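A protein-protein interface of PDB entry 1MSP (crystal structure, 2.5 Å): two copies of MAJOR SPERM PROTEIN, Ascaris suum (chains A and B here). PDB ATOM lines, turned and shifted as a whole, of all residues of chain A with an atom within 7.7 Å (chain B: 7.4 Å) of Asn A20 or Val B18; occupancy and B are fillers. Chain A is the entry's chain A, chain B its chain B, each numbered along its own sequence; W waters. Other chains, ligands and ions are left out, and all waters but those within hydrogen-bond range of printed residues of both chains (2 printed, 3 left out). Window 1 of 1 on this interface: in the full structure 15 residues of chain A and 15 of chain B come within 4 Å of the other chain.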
ATOM      1  N   LYS A  16      18.155  19.744 -24.546  1.00  0.00           N
ATOM      2  CA  LYS A  16      18.055  21.122 -24.152  1.00  0.00           C
ATOM      3  C   LYS A  16      17.209  21.381 -22.941  1.00  0.00           C
ATOM      4  O   LYS A  16      16.634  20.498 -22.332  1.00  0.00           O
ATOM      5  CB  LYS A  16      17.708  22.046 -25.279  1.00  0.00           C
ATOM      6  CG  LYS A  16      16.611  21.503 -26.167  1.00  0.00           C
ATOM      7  CD  LYS A  16      15.419  22.438 -26.154  1.00  0.00           C
ATOM      8  CE  LYS A  16      14.455  22.221 -27.305  1.00  0.00           C
ATOM      9  NZ  LYS A  16      14.152  23.464 -28.028  1.00  0.00           N
ATOM     10  N   ILE A  17      17.139  22.613 -22.554  1.00  0.00           N
ATOM     11  CA  ILE A  17      16.326  22.840 -21.422  1.00  0.00           C
ATOM     12  C   ILE A  17      15.570  24.147 -21.606  1.00  0.00           C
ATOM     13  O   ILE A  17      16.137  25.145 -22.076  1.00  0.00           O
ATOM     14  CB  ILE A  17      17.064  22.621 -20.120  1.00  0.00           C
ATOM     15  CG1 ILE A  17      16.075  22.785 -18.982  1.00  0.00           C
ATOM     16  CG2 ILE A  17      18.139  23.664 -19.968  1.00  0.00           C
ATOM     17  CD1 ILE A  17      16.729  23.384 -17.751  1.00  0.00           C
ATOM     18  N   VAL A  18      14.258  24.100 -21.304  1.00  0.00           N
ATOM     19  CA  VAL A  18      13.348  25.223 -21.468  1.00  0.00           C
ATOM     20  C   VAL A  18      12.809  25.827 -20.208  1.00  0.00           C
ATOM     21  O   VAL A  18      12.275  25.156 -19.345  1.00  0.00           O
ATOM     22  CB  VAL A  18      12.180  24.861 -22.336  1.00  0.00           C
ATOM     23  CG1 VAL A  18      11.425  26.167 -22.577  1.00  0.00           C
ATOM     24  CG2 VAL A  18      12.735  24.298 -23.647  1.00  0.00           C
ATOM     25  N   PHE A  19      12.988  27.117 -20.129  1.00  0.00           N
ATOM     26  CA  PHE A  19      12.525  27.892 -19.031  1.00  0.00           C
ATOM     27  C   PHE A  19      11.292  28.589 -19.574  1.00  0.00           C
ATOM     28  O   PHE A  19      11.306  29.165 -20.687  1.00  0.00           O
ATOM     29  CB  PHE A  19      13.609  28.899 -18.564  1.00  0.00           C
ATOM     30  CG  PHE A  19      14.777  28.231 -17.858  1.00  0.00           C
ATOM     31  CD1 PHE A  19      14.872  26.842 -17.818  1.00  0.00           C
ATOM     32  CD2 PHE A  19      15.797  28.947 -17.227  1.00  0.00           C
ATOM     33  CE1 PHE A  19      15.927  26.201 -17.173  1.00  0.00           C
ATOM     34  CE2 PHE A  19      16.868  28.321 -16.585  1.00  0.00           C
ATOM     35  CZ  PHE A  19      16.930  26.932 -16.545  1.00  0.00           C
ATOM     36  N   ASN A  20      10.216  28.514 -18.801  1.00  0.00           N
ATOM     37  CA  ASN A  20       8.938  29.085 -19.203  1.00  0.00           C
ATOM     38  C   ASN A  20       8.613  30.355 -18.464  1.00  0.00           C
ATOM     39  O   ASN A  20       8.799  30.382 -17.241  1.00  0.00           O
ATOM     40  CB  ASN A  20       7.847  28.071 -18.810  1.00  0.00           C
ATOM     41  CG  ASN A  20       7.602  27.008 -19.857  1.00  0.00           C
ATOM     42  OD1 ASN A  20       7.233  27.334 -20.994  1.00  0.00           O
ATOM     43  ND2 ASN A  20       7.755  25.733 -19.484  1.00  0.00           N
ATOM     44  N   ALA A  21       8.086  31.383 -19.167  1.00  0.00           N
ATOM     45  CA  ALA A  21       7.645  32.628 -18.494  1.00  0.00           C
ATOM     46  C   ALA A  21       6.532  32.239 -17.513  1.00  0.00           C
ATOM     47  O   ALA A  21       5.931  31.185 -17.662  1.00  0.00           O
ATOM     48  CB  ALA A  21       7.118  33.615 -19.523  1.00  0.00           C
ATOM     49  N   PRO A  22       6.191  33.033 -16.521  1.00  0.00           N
ATOM     50  CA  PRO A  22       6.750  34.316 -16.177  1.00  0.00           C
ATOM     51  C   PRO A  22       8.126  34.241 -15.451  1.00  0.00           C
ATOM     52  O   PRO A  22       8.411  33.330 -14.648  1.00  0.00           O
ATOM     53  CB  PRO A  22       5.742  34.866 -15.163  1.00  0.00           C
ATOM     54  CG  PRO A  22       5.045  33.664 -14.536  1.00  0.00           C
ATOM     55  CD  PRO A  22       5.267  32.509 -15.468  1.00  0.00           C
ATOM     56  N   TYR A  23       8.948  35.273 -15.720  1.00  0.00           N
ATOM     57  CA  TYR A  23      10.290  35.442 -15.172  1.00  0.00           C
ATOM     58  C   TYR A  23      10.410  36.426 -14.011  1.00  0.00           C
ATOM     59  O   TYR A  23      11.337  37.237 -13.954  1.00  0.00           O
ATOM     60  CB  TYR A  23      11.264  35.829 -16.291  1.00  0.00           C
ATOM     61  CG  TYR A  23      11.292  34.762 -17.350  1.00  0.00           C
ATOM     62  CD1 TYR A  23      11.487  33.438 -16.967  1.00  0.00           C
ATOM     63  CD2 TYR A  23      11.108  35.072 -18.697  1.00  0.00           C
ATOM     64  CE1 TYR A  23      11.520  32.434 -17.930  1.00  0.00           C
ATOM     65  CE2 TYR A  23      11.120  34.081 -19.677  1.00  0.00           C
ATOM     66  CZ  TYR A  23      11.332  32.763 -19.272  1.00  0.00           C
ATOM     67  OH  TYR A  23      11.369  31.767 -20.201  1.00  0.00           O
ATOM     68  N   ASP A  24       9.481  36.368 -13.070  1.00  0.00           N
ATOM     69  CA  ASP A  24       9.540  37.278 -11.953  1.00  0.00           C
ATOM     70  C   ASP A  24       9.670  36.506 -10.683  1.00  0.00           C
ATOM     71  O   ASP A  24       9.619  37.028  -9.575  1.00  0.00           O
ATOM     72  CB  ASP A  24       8.422  38.342 -11.901  1.00  0.00           C
ATOM     73  CG  ASP A  24       7.059  37.873 -12.338  1.00  0.00           C
ATOM     74  OD1 ASP A  24       6.396  37.031 -11.729  1.00  0.00           O
ATOM     75  OD2 ASP A  24       6.672  38.498 -13.433  1.00  0.00           O
ATOM     76  N   ASP A  25       9.858  35.236 -10.895  1.00  0.00           N
ATOM     77  CA  ASP A  25      10.027  34.362  -9.775  1.00  0.00           C
ATOM     78  C   ASP A  25      11.288  33.505  -9.984  1.00  0.00           C
ATOM     79  O   ASP A  25      11.746  33.293 -11.117  1.00  0.00           O
ATOM     80  CB  ASP A  25       8.743  33.536  -9.560  1.00  0.00           C
ATOM     81  N   HIS A  27      12.713  30.419 -10.600  1.00  0.00           N
ATOM     82  CA  HIS A  27      12.339  29.123 -11.153  1.00  0.00           C
ATOM     83  C   HIS A  27      13.459  28.048 -11.088  1.00  0.00           C
ATOM     84  O   HIS A  27      14.464  28.126 -11.790  1.00  0.00           O
ATOM     85  CB  HIS A  27      11.688  29.284 -12.566  1.00  0.00           C
ATOM     86  N   TYR A  29      14.377  24.327 -12.002  1.00  0.00           N
ATOM     87  CA  TYR A  29      14.152  23.060 -12.711  1.00  0.00           C
ATOM     88  C   TYR A  29      15.100  21.989 -12.175  1.00  0.00           C
ATOM     89  O   TYR A  29      15.715  22.187 -11.138  1.00  0.00           O
ATOM     90  CB  TYR A  29      14.356  23.232 -14.219  1.00  0.00           C
ATOM     91  CG  TYR A  29      13.480  24.315 -14.789  1.00  0.00           C
ATOM     92  CD1 TYR A  29      13.567  25.658 -14.407  1.00  0.00           C
ATOM     93  CD2 TYR A  29      12.538  23.963 -15.751  1.00  0.00           C
ATOM     94  CE1 TYR A  29      12.713  26.625 -14.949  1.00  0.00           C
ATOM     95  CE2 TYR A  29      11.686  24.911 -16.310  1.00  0.00           C
ATOM     96  CZ  TYR A  29      11.763  26.240 -15.898  1.00  0.00           C
ATOM     97  OH  TYR A  29      10.923  27.180 -16.448  1.00  0.00           O
ATOM     98  N   GLU A 123      16.591  27.335 -23.517  1.00  0.00           N
ATOM     99  CA  GLU A 123      15.603  27.945 -24.377  1.00  0.00           C
ATOM    100  C   GLU A 123      14.614  28.658 -23.503  1.00  0.00           C
ATOM    101  O   GLU A 123      14.045  28.074 -22.584  1.00  0.00           O
ATOM    102  CB  GLU A 123      14.870  26.973 -25.305  1.00  0.00           C
ATOM    103  CG  GLU A 123      14.410  27.572 -26.647  1.00  0.00           C
ATOM    104  CD  GLU A 123      13.759  26.514 -27.487  1.00  0.00           C
ATOM    105  OE1 GLU A 123      14.617  25.716 -28.077  1.00  0.00           O
ATOM    106  OE2 GLU A 123      12.556  26.390 -27.570  1.00  0.00           O
ATOM    107  N   TYR A 124      14.410  29.917 -23.780  1.00  0.00           N
ATOM    108  CA  TYR A 124      13.440  30.672 -23.010  1.00  0.00           C
ATOM    109  C   TYR A 124      12.058  30.750 -23.689  1.00  0.00           C
ATOM    110  O   TYR A 124      11.925  31.258 -24.807  1.00  0.00           O
ATOM    111  CB  TYR A 124      13.986  32.064 -22.856  1.00  0.00           C
ATOM    112  CG  TYR A 124      15.213  32.064 -22.022  1.00  0.00           C
ATOM    113  CD1 TYR A 124      15.104  31.975 -20.635  1.00  0.00           C
ATOM    114  CD2 TYR A 124      16.464  32.197 -22.616  1.00  0.00           C
ATOM    115  CE1 TYR A 124      16.223  32.037 -19.812  1.00  0.00           C
ATOM    116  CE2 TYR A 124      17.592  32.251 -21.804  1.00  0.00           C
ATOM    117  CZ  TYR A 124      17.470  32.177 -20.415  1.00  0.00           C
ATOM    118  OH  TYR A 124      18.592  32.234 -19.635  1.00  0.00           O
ATOM    119  N   ASN A 125      11.030  30.235 -23.031  1.00  0.00           N
ATOM    120  CA  ASN A 125       9.708  30.284 -23.634  1.00  0.00           C
ATOM    121  C   ASN A 125       8.864  31.394 -23.042  1.00  0.00           C
ATOM    122  O   ASN A 125       8.487  31.325 -21.865  1.00  0.00           O
ATOM    123  CB  ASN A 125       8.971  28.974 -23.380  1.00  0.00           C
ATOM    124  CG  ASN A 125       7.664  28.969 -24.112  1.00  0.00           C
ATOM    125  OD1 ASN A 125       7.558  29.470 -25.238  1.00  0.00           O
ATOM    126  ND2 ASN A 125       6.674  28.381 -23.479  1.00  0.00           N
ATOM    127  N   LEU A 126       8.585  32.410 -23.841  1.00  0.00           N
ATOM    128  CA  LEU A 126       7.816  33.542 -23.348  1.00  0.00           C
ATOM    129  C   LEU A 126       6.310  33.429 -23.402  1.00  0.00           C
ATOM    130  O   LEU A 126       5.699  33.707 -22.343  1.00  0.00           O
ATOM    131  CB  LEU A 126       8.176  34.770 -24.142  1.00  0.00           C
ATOM    132  CG  LEU A 126       9.547  35.293 -23.815  1.00  0.00           C
ATOM    133  CD1 LEU A 126       9.557  36.690 -24.400  1.00  0.00           C
ATOM    134  CD2 LEU A 126       9.765  35.338 -22.300  1.00  0.00           C
ATOM    135  OXT LEU A 126       5.799  33.145 -24.517  1.00  0.00           O
ATOM    136  N   GLN B  12       1.130  34.409 -19.522  1.00  0.00           N
ATOM    137  CA  GLN B  12       2.580  34.231 -19.386  1.00  0.00           C
ATOM    138  C   GLN B  12       2.782  32.793 -18.854  1.00  0.00           C
ATOM    139  O   GLN B  12       2.434  32.487 -17.706  1.00  0.00           O
ATOM    140  CB  GLN B  12       3.192  35.276 -18.403  1.00  0.00           C
ATOM    141  CG  GLN B  12       3.835  36.541 -19.032  1.00  0.00           C
ATOM    142  CD  GLN B  12       4.150  37.626 -17.981  1.00  0.00           C
ATOM    143  OE1 GLN B  12       4.179  37.366 -16.770  1.00  0.00           O
ATOM    144  NE2 GLN B  12       4.381  38.870 -18.415  1.00  0.00           N
ATOM    145  N   PRO B  13       3.275  31.837 -19.644  1.00  0.00           N
ATOM    146  CA  PRO B  13       3.791  31.916 -21.007  1.00  0.00           C
ATOM    147  C   PRO B  13       2.723  32.346 -21.983  1.00  0.00           C
ATOM    148  O   PRO B  13       1.547  32.100 -21.764  1.00  0.00           O
ATOM    149  CB  PRO B  13       4.362  30.529 -21.317  1.00  0.00           C
ATOM    150  CG  PRO B  13       4.351  29.753 -19.999  1.00  0.00           C
ATOM    151  CD  PRO B  13       3.480  30.522 -19.009  1.00  0.00           C
ATOM    152  N   SER B  14       3.122  32.979 -23.062  1.00  0.00           N
ATOM    153  CA  SER B  14       2.127  33.476 -23.981  1.00  0.00           C
ATOM    154  C   SER B  14       1.539  32.492 -24.973  1.00  0.00           C
ATOM    155  O   SER B  14       0.451  32.694 -25.473  1.00  0.00           O
ATOM    156  CB  SER B  14       2.622  34.710 -24.715  1.00  0.00           C
ATOM    157  OG  SER B  14       3.079  34.349 -26.007  1.00  0.00           O
ATOM    158  N   LYS B  16       2.679  28.694 -25.140  1.00  0.00           N
ATOM    159  CA  LYS B  16       2.693  27.280 -24.791  1.00  0.00           C
ATOM    160  C   LYS B  16       3.351  27.054 -23.462  1.00  0.00           C
ATOM    161  O   LYS B  16       3.950  27.961 -22.899  1.00  0.00           O
ATOM    162  CB  LYS B  16       3.352  26.430 -25.866  1.00  0.00           C
ATOM    163  CG  LYS B  16       4.712  25.899 -25.458  1.00  0.00           C
ATOM    164  CD  LYS B  16       5.835  26.598 -26.202  1.00  0.00           C
ATOM    165  CE  LYS B  16       5.913  26.222 -27.669  1.00  0.00           C
ATOM    166  NZ  LYS B  16       6.773  27.134 -28.437  1.00  0.00           N
ATOM    167  N   ILE B  17       3.220  25.861 -22.948  1.00  0.00           N
ATOM    168  CA  ILE B  17       3.849  25.545 -21.688  1.00  0.00           C
ATOM    169  C   ILE B  17       4.693  24.370 -21.994  1.00  0.00           C
ATOM    170  O   ILE B  17       4.174  23.450 -22.645  1.00  0.00           O
ATOM    171  CB  ILE B  17       2.911  25.103 -20.606  1.00  0.00           C
ATOM    172  CG1 ILE B  17       1.974  26.248 -20.360  1.00  0.00           C
ATOM    173  CG2 ILE B  17       3.687  24.808 -19.323  1.00  0.00           C
ATOM    174  CD1 ILE B  17       1.890  26.541 -18.877  1.00  0.00           C
ATOM    175  N   VAL B  18       5.970  24.446 -21.550  1.00  0.00           N
ATOM    176  CA  VAL B  18       6.949  23.392 -21.773  1.00  0.00           C
ATOM    177  C   VAL B  18       7.377  22.624 -20.560  1.00  0.00           C
ATOM    178  O   VAL B  18       7.863  23.151 -19.562  1.00  0.00           O
ATOM    179  CB  VAL B  18       8.041  23.631 -22.801  1.00  0.00           C
ATOM    180  CG1 VAL B  18       8.408  22.287 -23.355  1.00  0.00           C
ATOM    181  CG2 VAL B  18       7.498  24.466 -23.961  1.00  0.00           C
ATOM    182  N   PHE B  19       7.160  21.344 -20.665  1.00  0.00           N
ATOM    183  CA  PHE B  19       7.514  20.481 -19.574  1.00  0.00           C
ATOM    184  C   PHE B  19       8.820  19.729 -19.851  1.00  0.00           C
ATOM    185  O   PHE B  19       8.955  19.008 -20.831  1.00  0.00           O
ATOM    186  CB  PHE B  19       6.377  19.468 -19.404  1.00  0.00           C
ATOM    187  CG  PHE B  19       5.153  20.036 -18.773  1.00  0.00           C
ATOM    188  CD1 PHE B  19       5.204  20.979 -17.748  1.00  0.00           C
ATOM    189  CD2 PHE B  19       3.902  19.588 -19.185  1.00  0.00           C
ATOM    190  CE1 PHE B  19       4.052  21.484 -17.139  1.00  0.00           C
ATOM    191  CE2 PHE B  19       2.739  20.088 -18.596  1.00  0.00           C
ATOM    192  CZ  PHE B  19       2.810  21.028 -17.571  1.00  0.00           C
ATOM    193  N   ASN B  20       9.790  19.833 -18.972  1.00  0.00           N
ATOM    194  CA  ASN B  20      11.042  19.147 -19.219  1.00  0.00           C
ATOM    195  C   ASN B  20      11.180  17.820 -18.491  1.00  0.00           C
ATOM    196  O   ASN B  20      10.717  17.708 -17.357  1.00  0.00           O
ATOM    197  CB  ASN B  20      12.167  20.050 -18.679  1.00  0.00           C
ATOM    198  CG  ASN B  20      12.180  21.431 -19.282  1.00  0.00           C
ATOM    199  OD1 ASN B  20      12.668  21.620 -20.398  1.00  0.00           O
ATOM    200  ND2 ASN B  20      11.712  22.418 -18.525  1.00  0.00           N
ATOM    201  N   TYR B  23      10.590  12.762 -15.858  1.00  0.00           N
ATOM    202  CA  TYR B  23       9.164  12.651 -15.496  1.00  0.00           C
ATOM    203  C   TYR B  23       8.925  11.614 -14.420  1.00  0.00           C
ATOM    204  O   TYR B  23       7.935  10.887 -14.443  1.00  0.00           O
ATOM    205  CB  TYR B  23       8.311  12.193 -16.707  1.00  0.00           C
ATOM    206  CG  TYR B  23       8.385  13.214 -17.811  1.00  0.00           C
ATOM    207  CD1 TYR B  23       7.910  14.502 -17.593  1.00  0.00           C
ATOM    208  CD2 TYR B  23       9.005  12.976 -19.032  1.00  0.00           C
ATOM    209  CE1 TYR B  23       7.986  15.507 -18.553  1.00  0.00           C
ATOM    210  CE2 TYR B  23       9.089  13.967 -20.015  1.00  0.00           C
ATOM    211  CZ  TYR B  23       8.575  15.239 -19.782  1.00  0.00           C
ATOM    212  OH  TYR B  23       8.621  16.218 -20.747  1.00  0.00           O
ATOM    213  N   TYR B  29       4.321  23.638 -12.556  1.00  0.00           N
ATOM    214  CA  TYR B  29       4.602  24.810 -13.323  1.00  0.00           C
ATOM    215  C   TYR B  29       3.567  25.814 -12.837  1.00  0.00           C
ATOM    216  O   TYR B  29       2.729  25.490 -11.997  1.00  0.00           O
ATOM    217  CB  TYR B  29       4.621  24.592 -14.853  1.00  0.00           C
ATOM    218  CG  TYR B  29       5.825  23.773 -15.242  1.00  0.00           C
ATOM    219  CD1 TYR B  29       5.943  22.472 -14.758  1.00  0.00           C
ATOM    220  CD2 TYR B  29       6.845  24.275 -16.057  1.00  0.00           C
ATOM    221  CE1 TYR B  29       7.058  21.698 -15.079  1.00  0.00           C
ATOM    222  CE2 TYR B  29       7.957  23.505 -16.401  1.00  0.00           C
ATOM    223  CZ  TYR B  29       8.068  22.207 -15.899  1.00  0.00           C
ATOM    224  OH  TYR B  29       9.168  21.439 -16.221  1.00  0.00           O
ATOM    225  N   HIS B  30       3.634  27.026 -13.326  1.00  0.00           N
ATOM    226  CA  HIS B  30       2.748  28.054 -12.896  1.00  0.00           C
ATOM    227  C   HIS B  30       2.425  28.978 -14.063  1.00  0.00           C
ATOM    228  O   HIS B  30       3.257  29.174 -14.937  1.00  0.00           O
ATOM    229  CB  HIS B  30       3.474  28.768 -11.751  1.00  0.00           C
ATOM    230  CG  HIS B  30       3.325  28.041 -10.457  1.00  0.00           C
ATOM    231  ND1 HIS B  30       4.321  28.014  -9.506  1.00  0.00           N
ATOM    232  CD2 HIS B  30       2.271  27.351  -9.958  1.00  0.00           C
ATOM    233  CE1 HIS B  30       3.860  27.300  -8.470  1.00  0.00           C
ATOM    234  NE2 HIS B  30       2.626  26.886  -8.705  1.00  0.00           N
ATOM    235  N   PRO B 121      -1.295  24.831 -25.615  1.00  0.00           N
ATOM    236  CA  PRO B 121      -0.872  23.467 -25.702  1.00  0.00           C
ATOM    237  C   PRO B 121       0.377  23.234 -24.831  1.00  0.00           C
ATOM    238  O   PRO B 121       1.146  24.166 -24.547  1.00  0.00           O
ATOM    239  CB  PRO B 121      -0.504  23.253 -27.159  1.00  0.00           C
ATOM    240  CG  PRO B 121      -0.506  24.617 -27.837  1.00  0.00           C
ATOM    241  CD  PRO B 121      -0.920  25.633 -26.793  1.00  0.00           C
ATOM    242  N   ILE B 122       0.545  21.972 -24.427  1.00  0.00           N
ATOM    243  CA  ILE B 122       1.639  21.476 -23.638  1.00  0.00           C
ATOM    244  C   ILE B 122       2.645  20.821 -24.581  1.00  0.00           C
ATOM    245  O   ILE B 122       2.251  20.055 -25.476  1.00  0.00           O
ATOM    246  CB  ILE B 122       1.151  20.385 -22.704  1.00  0.00           C
ATOM    247  CG1 ILE B 122      -0.101  20.829 -21.976  1.00  0.00           C
ATOM    248  CG2 ILE B 122       2.238  19.952 -21.716  1.00  0.00           C
ATOM    249  CD1 ILE B 122       0.189  21.411 -20.608  1.00  0.00           C
ATOM    250  N   GLU B 123       3.931  21.144 -24.346  1.00  0.00           N
ATOM    251  CA  GLU B 123       5.092  20.615 -25.044  1.00  0.00           C
ATOM    252  C   GLU B 123       5.958  19.879 -24.020  1.00  0.00           C
ATOM    253  O   GLU B 123       6.258  20.366 -22.927  1.00  0.00           O
ATOM    254  CB  GLU B 123       5.867  21.688 -25.814  1.00  0.00           C
ATOM    255  CG  GLU B 123       6.433  21.174 -27.150  1.00  0.00           C
ATOM    256  CD  GLU B 123       7.240  22.186 -27.926  1.00  0.00           C
ATOM    257  OE1 GLU B 123       8.429  22.370 -27.739  1.00  0.00           O
ATOM    258  OE2 GLU B 123       6.519  22.836 -28.814  1.00  0.00           O
ATOM    259  N   TYR B 124       6.283  18.659 -24.367  1.00  0.00           N
ATOM    260  CA  TYR B 124       7.084  17.792 -23.548  1.00  0.00           C
ATOM    261  C   TYR B 124       8.498  17.709 -24.092  1.00  0.00           C
ATOM    262  O   TYR B 124       8.694  17.230 -25.195  1.00  0.00           O
ATOM    263  CB  TYR B 124       6.515  16.376 -23.619  1.00  0.00           C
ATOM    264  CG  TYR B 124       5.190  16.337 -22.950  1.00  0.00           C
ATOM    265  CD1 TYR B 124       5.144  16.322 -21.556  1.00  0.00           C
ATOM    266  CD2 TYR B 124       4.007  16.338 -23.695  1.00  0.00           C
ATOM    267  CE1 TYR B 124       3.916  16.305 -20.901  1.00  0.00           C
ATOM    268  CE2 TYR B 124       2.773  16.323 -23.048  1.00  0.00           C
ATOM    269  CZ  TYR B 124       2.739  16.311 -21.650  1.00  0.00           C
ATOM    270  OH  TYR B 124       1.543  16.269 -20.983  1.00  0.00           O
ATOM    271  N   ASN B 125       9.487  18.165 -23.336  1.00  0.00           N
ATOM    272  CA  ASN B 125      10.888  18.099 -23.750  1.00  0.00           C
ATOM    273  C   ASN B 125      11.525  16.906 -23.147  1.00  0.00           C
ATOM    274  O   ASN B 125      11.651  16.880 -21.928  1.00  0.00           O
ATOM    275  CB  ASN B 125      11.646  19.146 -22.982  1.00  0.00           C
ATOM    276  CG  ASN B 125      12.927  19.453 -23.676  1.00  0.00           C
ATOM    277  OD1 ASN B 125      13.201  18.962 -24.769  1.00  0.00           O
ATOM    278  ND2 ASN B 125      13.639  20.360 -23.068  1.00  0.00           N
ATOM    279  N   LEU B 126      11.934  15.956 -23.961  1.00  0.00           N
ATOM    280  CA  LEU B 126      12.534  14.737 -23.472  1.00  0.00           C
ATOM    281  C   LEU B 126      14.046  14.823 -23.239  1.00  0.00           C
ATOM    282  O   LEU B 126      14.743  15.281 -24.175  1.00  0.00           O
ATOM    283  CB  LEU B 126      12.110  13.538 -24.317  1.00  0.00           C
ATOM    284  CG  LEU B 126      10.602  13.396 -24.318  1.00  0.00           C
ATOM    285  CD1 LEU B 126      10.117  12.739 -25.608  1.00  0.00           C
ATOM    286  CD2 LEU B 126      10.201  12.564 -23.108  1.00  0.00           C
ATOM    287  OXT LEU B 126      14.510  14.437 -22.135  1.00  0.00           O
HETATM  288  O   HOH W   1      15.716  17.534 -24.613  1.00  0.00           O
HETATM  289  O   HOH W   2       5.005  30.783 -25.367  1.00  0.00           O
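The backbone carbonyl oxygen (O) of Lys A16 lies within hydrogen-bond range of the side-chain amide nitrogen (ND2) of Asn B125, 3.1 Å away.
The backbone carbonyl oxygen (O) of Val A18 is in hydrogen-bond range of the side-chain amide nitrogen (ND2) of Asn B20 (2.9 Å).
The side-chain amide nitrogen (ND2) of Asn A20 sits at hydrogen-bond distance from the backbone carbonyl oxygen (O) of Val B18, at 2.6 Å.
ND2 of Asn A125 sits at hydrogen-bond distance from O of Lys B16 (2.8 Å).
The chain-end carboxylate of Leu A126 is in hydrogen-bond range of the backbone NH of Ser B14 (2.8 Å).
The backbone nitrogen (N) of Pro B13 sits close to the backbone carbonyl oxygen (O) of Ala A21 (3.4 Å).
The side-chain hydroxyl (OH) of Tyr A29 sits at hydrogen-bond distance from the backbone NH (N) of Asn A20 (2.8 Å).
OD1 of Asn A20 is in hydrogen-bond range of ND2 of Asn A125, 2.8 Å away.
N of Ala A21 lies within hydrogen-bond range of OH of Tyr A23 (3.5 Å).
The backbone carbonyl oxygen of Asn A125 lies within hydrogen-bond range of the backbone NH of Ala A21, at 2.7 Å.
The backbone NH of Asn A125 lies within hydrogen-bond range of the side-chain hydroxyl of Tyr A23 (3.2 Å).
The backbone carbonyl oxygen (O) of Phe B19 sits at hydrogen-bond distance from the backbone NH (N) of Asn B125, at 2.7 Å.
Among the printed residues, merely in contact across the chains: Ile A17 with Asn B20 (3.9 Å), Asn A20 with Pro B13 (3.9 Å), Asn A20 with Lys B16 (3.8 Å), Asn A20 with Ile B17 (3.9 Å), Asn A20 with Tyr B29 (3.8 Å), Ala A21 with Gln B12 (3.7 Å), Pro A22 with Gln B12 (3.4 Å), Pro A22 with His B30 (3.9 Å), Tyr A29 with Asn B20 (3.3 Å), Tyr A29 with Tyr B29 (3.99 Å), Asn A125 with Pro B13 (3.8 Å) and Leu A126 with Pro B13 (2.9 Å).
Of chain B, only Pro B13 (3.9 Å), Lys B16 (3.8 Å), Ile B17 (3.9 Å), Val B18 (2.6 Å) and Tyr B29 (3.8 Å) come within 4 Å of Asn A20.
Of chain A, only Asn A20 comes within 4 Å of Val B18.
Printed residues of chain A within 4 Å of Ser B14: Leu A126.
Of the printed residues of chain A, Tyr B29 touches Asn A20 and Tyr A29.
Of the printed residues of chain A, Ile B17 touches Asn A20.
Of the 16 printed residues of chain A, 9 touch a printed residue of chain B.
Printed residues of chain A that touch a printed residue of chain B: Lys A16, Ile A17, Val A18, Asn A20, Ala A21, Pro A22, Tyr A29, Asn A125 and Leu A126.
Hydrophobic or aromatic side chains of chain A that line the printed part of chain B: Ile A17, Val A18, Pro A22 and Tyr A29.
Along chain A the printed residues that touch a printed residue of chain B span positions 16 to 126.
Among the printed residues, 18 pairs touch across the chains.
Among the printed residues, no Asp or Glu carboxylate lies within 4 Å of a Lys or Arg side-chain nitrogen of the other chain.
Lys A16 touches Asn B125, and with the chains exchanged Asn A125 touches Lys B16.
Ile A17 touches Asn B20, and with the chains exchanged Asn A20 touches Ile B17.
Asn A20 touches Tyr B29, and with the chains exchanged Tyr A29 touches Asn B20.
Tyr B29 touches its own counterpart, Tyr A29.
Of the 18 pairs that touch across the chains among the printed residues, 9 have their exchanged pair printed and touching as well.
Water W1 lies within hydrogen-bond range of O of Leu B126 (2.5 Å), OD1 of Asn B125 (2.9 Å) and N of Lys A16 (3.3 Å).
Water W2 lies within hydrogen-bond range of OXT of Leu A126 (2.6 Å), OD1 of Asn A125 (2.9 Å) and N of Lys B16 (3.1 Å).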
